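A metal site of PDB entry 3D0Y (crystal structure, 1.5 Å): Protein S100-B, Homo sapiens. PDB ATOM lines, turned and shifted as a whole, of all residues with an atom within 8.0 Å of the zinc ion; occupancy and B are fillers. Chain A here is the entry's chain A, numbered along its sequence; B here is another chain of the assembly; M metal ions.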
ATOM      1  N   HIS A  86      25.245  -9.668 -10.600  1.00  0.00           N
ATOM      2  CA  HIS A  86      25.844  -8.473 -10.052  1.00  0.00           C
ATOM      3  C   HIS A  86      26.731  -8.801  -8.859  1.00  0.00           C
ATOM      4  O   HIS A  86      27.933  -8.510  -8.893  1.00  0.00           O
ATOM      5  CB  HIS A  86      24.754  -7.456  -9.659  1.00  0.00           C
ATOM      6  CG  HIS A  86      25.319  -6.191  -9.117  1.00  0.00           C
ATOM      7  ND1 HIS A  86      24.943  -5.657  -7.904  1.00  0.00           N
ATOM      8  CD2 HIS A  86      26.256  -5.349  -9.616  1.00  0.00           C
ATOM      9  CE1 HIS A  86      25.624  -4.546  -7.680  1.00  0.00           C
ATOM     10  NE2 HIS A  86      26.418  -4.329  -8.709  1.00  0.00           N
ATOM     11  N   GLU A  87      26.174  -9.439  -7.846  1.00  0.00           N
ATOM     12  CA  GLU A  87      26.881  -9.744  -6.614  1.00  0.00           C
ATOM     13  C   GLU A  87      27.994 -10.742  -6.823  1.00  0.00           C
ATOM     14  O   GLU A  87      29.074 -10.582  -6.276  1.00  0.00           O
ATOM     15  CB  GLU A  87      25.943 -10.334  -5.503  1.00  0.00           C
ATOM     16  CG  GLU A  87      24.509  -9.762  -5.370  1.00  0.00           C
ATOM     17  CD  GLU A  87      24.431  -8.406  -4.703  1.00  0.00           C
ATOM     18  OE1 GLU A  87      25.431  -7.678  -4.734  1.00  0.00           O
ATOM     19  OE2 GLU A  87      23.328  -8.069  -4.162  1.00  0.00           O
ATOM     20  N   PHE A  89      29.828 -11.607  -9.351  1.00  0.00           N
ATOM     21  CA  PHE A  89      30.974 -11.268 -10.182  1.00  0.00           C
ATOM     22  C   PHE A  89      31.789 -10.075  -9.664  1.00  0.00           C
ATOM     23  O   PHE A  89      32.779  -9.665 -10.258  1.00  0.00           O
ATOM     24  CB  PHE A  89      30.536 -11.135 -11.635  1.00  0.00           C
ATOM     25  CG  PHE A  89      30.244 -12.469 -12.324  1.00  0.00           C
ATOM     26  CD1 PHE A  89      28.975 -12.789 -12.763  1.00  0.00           C
ATOM     27  CD2 PHE A  89      31.286 -13.392 -12.513  1.00  0.00           C
ATOM     28  CE1 PHE A  89      28.717 -14.025 -13.397  1.00  0.00           C
ATOM     29  CE2 PHE A  89      31.047 -14.623 -13.136  1.00  0.00           C
ATOM     30  CZ  PHE A  89      29.749 -14.926 -13.579  1.00  0.00           C
ATOM     31  N   GLU A  90      31.417  -9.554  -8.506  1.00  0.00           N
ATOM     32  CA  GLU A  90      32.177  -8.475  -7.907  1.00  0.00           C
ATOM     33  C   GLU A  90      32.941  -9.049  -6.753  1.00  0.00           C
ATOM     34  O   GLU A  90      32.423  -9.971  -6.116  1.00  0.00           O
ATOM     35  CB  GLU A  90      31.236  -7.354  -7.450  1.00  0.00           C
ATOM     36  CG  GLU A  90      30.601  -6.673  -8.609  1.00  0.00           C
ATOM     37  CD  GLU A  90      29.835  -5.403  -8.303  1.00  0.00           C
ATOM     38  OE1 GLU A  90      29.555  -4.692  -9.276  1.00  0.00           O
ATOM     39  OE2 GLU A  90      29.459  -5.108  -7.154  1.00  0.00           O
ATOM     40  N   ILE B  12      23.352  -4.202 -15.696  1.00  0.00           N
ATOM     41  CA  ILE B  12      24.401  -4.008 -14.708  1.00  0.00           C
ATOM     42  C   ILE B  12      25.401  -2.947 -15.245  1.00  0.00           C
ATOM     43  O   ILE B  12      25.793  -2.024 -14.511  1.00  0.00           O
ATOM     44  CB  ILE B  12      25.094  -5.314 -14.448  1.00  0.00           C
ATOM     45  CG1 ILE B  12      24.133  -6.375 -13.832  1.00  0.00           C
ATOM     46  CG2 ILE B  12      26.331  -5.081 -13.652  1.00  0.00           C
ATOM     47  CD1 ILE B  12      24.664  -7.779 -13.997  1.00  0.00           C
ATOM     48  N   PHE B  15      23.876   0.702 -15.161  1.00  0.00           N
ATOM     49  CA  PHE B  15      23.852   1.088 -13.746  1.00  0.00           C
ATOM     50  C   PHE B  15      25.230   1.531 -13.243  1.00  0.00           C
ATOM     51  O   PHE B  15      25.360   2.618 -12.673  1.00  0.00           O
ATOM     52  CB  PHE B  15      23.268  -0.016 -12.829  1.00  0.00           C
ATOM     53  CG  PHE B  15      23.289   0.352 -11.354  1.00  0.00           C
ATOM     54  CD1 PHE B  15      22.299   1.137 -10.797  1.00  0.00           C
ATOM     55  CD2 PHE B  15      24.363  -0.044 -10.539  1.00  0.00           C
ATOM     56  CE1 PHE B  15      22.375   1.494  -9.406  1.00  0.00           C
ATOM     57  CE2 PHE B  15      24.455   0.302  -9.163  1.00  0.00           C
ATOM     58  CZ  PHE B  15      23.440   1.060  -8.597  1.00  0.00           C
ATOM     59  N   HIS B  16      26.240   0.684 -13.482  1.00  0.00           N
ATOM     60  CA  HIS B  16      27.616   1.023 -13.121  1.00  0.00           C
ATOM     61  C   HIS B  16      28.091   2.296 -13.830  1.00  0.00           C
ATOM     62  O   HIS B  16      28.710   3.135 -13.212  1.00  0.00           O
ATOM     63  CB  HIS B  16      28.526  -0.161 -13.447  1.00  0.00           C
ATOM     64  CG  HIS B  16      28.542  -1.228 -12.402  1.00  0.00           C
ATOM     65  ND1 HIS B  16      28.603  -2.581 -12.713  1.00  0.00           N
ATOM     66  CD2 HIS B  16      28.596  -1.161 -11.043  1.00  0.00           C
ATOM     67  CE1 HIS B  16      28.628  -3.289 -11.596  1.00  0.00           C
ATOM     68  NE2 HIS B  16      28.659  -2.454 -10.573  1.00  0.00           N
ATOM     69  N   SER B  19      26.265   5.140 -11.829  1.00  0.00           N
ATOM     70  CA  SER B  19      26.439   5.102 -10.360  1.00  0.00           C
ATOM     71  C   SER B  19      27.872   5.449  -9.990  1.00  0.00           C
ATOM     72  O   SER B  19      28.160   5.925  -8.879  1.00  0.00           O
ATOM     73  CB  SER B  19      25.980   3.756  -9.804  1.00  0.00           C
ATOM     74  OG  SER B  19      26.981   2.750 -10.007  1.00  0.00           O
ATOM     75  N   LYS B  25      30.077   5.029  -5.423  1.00  0.00           N
ATOM     76  CA  LYS B  25      30.387   4.518  -6.763  1.00  0.00           C
ATOM     77  C   LYS B  25      29.437   3.404  -7.206  1.00  0.00           C
ATOM     78  O   LYS B  25      29.465   2.987  -8.345  1.00  0.00           O
ATOM     79  CB  LYS B  25      31.870   4.048  -6.821  1.00  0.00           C
ATOM     80  N   HIS B  26      28.549   2.996  -6.280  1.00  0.00           N
ATOM     81  CA  HIS B  26      27.720   1.829  -6.393  1.00  0.00           C
ATOM     82  C   HIS B  26      26.260   2.175  -6.165  1.00  0.00           C
ATOM     83  O   HIS B  26      25.412   1.298  -6.042  1.00  0.00           O
ATOM     84  CB  HIS B  26      28.159   0.832  -5.329  1.00  0.00           C
ATOM     85  CG  HIS B  26      28.258  -0.575  -5.826  1.00  0.00           C
ATOM     86  ND1 HIS B  26      28.144  -1.676  -4.991  1.00  0.00           N
ATOM     87  CD2 HIS B  26      28.521  -1.060  -7.065  1.00  0.00           C
ATOM     88  CE1 HIS B  26      28.312  -2.776  -5.705  1.00  0.00           C
ATOM     89  NE2 HIS B  26      28.531  -2.430  -6.970  1.00  0.00           N
ATOM     90  N   LYS B  27      25.990   3.464  -6.087  1.00  0.00           N
ATOM     91  CA  LYS B  27      24.607   3.931  -6.019  1.00  0.00           C
ATOM     92  C   LYS B  27      24.443   5.159  -6.879  1.00  0.00           C
ATOM     93  O   LYS B  27      25.436   5.848  -7.133  1.00  0.00           O
ATOM     94  CB  LYS B  27      24.232   4.265  -4.571  1.00  0.00           C
ATOM     95  CG  LYS B  27      24.405   3.134  -3.612  1.00  0.00           C
ATOM     96  CD  LYS B  27      23.660   3.487  -2.381  1.00  0.00           C
ATOM     97  CE  LYS B  27      23.860   2.397  -1.383  1.00  0.00           C
ATOM     98  NZ  LYS B  27      25.343   2.275  -0.928  1.00  0.00           N
ATOM     99  N   PHE B  71      21.428  -0.813  -6.526  1.00  0.00           N
ATOM    100  CA  PHE B  71      21.119  -1.716  -7.660  1.00  0.00           C
ATOM    101  C   PHE B  71      19.745  -2.367  -7.594  1.00  0.00           C
ATOM    102  O   PHE B  71      19.021  -2.400  -8.615  1.00  0.00           O
ATOM    103  CB  PHE B  71      22.174  -2.828  -7.847  1.00  0.00           C
ATOM    104  CG  PHE B  71      22.024  -3.532  -9.162  1.00  0.00           C
ATOM    105  CD1 PHE B  71      22.264  -2.858 -10.372  1.00  0.00           C
ATOM    106  CD2 PHE B  71      21.623  -4.866  -9.202  1.00  0.00           C
ATOM    107  CE1 PHE B  71      22.111  -3.482 -11.595  1.00  0.00           C
ATOM    108  CE2 PHE B  71      21.475  -5.512 -10.423  1.00  0.00           C
ATOM    109  CZ  PHE B  71      21.717  -4.828 -11.632  1.00  0.00           C
HETATM  110 ZN    ZN M   1      28.294  -3.206  -8.724  1.00  0.00          ZN
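A ring nitrogen (ND1) of His 16 of chain B sits at hydrogen-bond distance from the backbone carbonyl oxygen (O) of Ile 12 of chain B, at 3.4 Å.
Along chain A the residues within 4 Å of the zinc ion span positions 86 to 90.
The zinc ion is bound by a ring nitrogen (NE2) of His 26 of chain B (1.9 Å), the side-chain carboxylate (OE1) of Glu 90 (2.0 Å), a ring nitrogen (NE2) of His 16 of chain B (2.0 Å) and a ring nitrogen (NE2) of His 86 (2.2 Å).
Slightly farther from the zinc ion lies OE2 of Glu 90 (2.7 Å).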
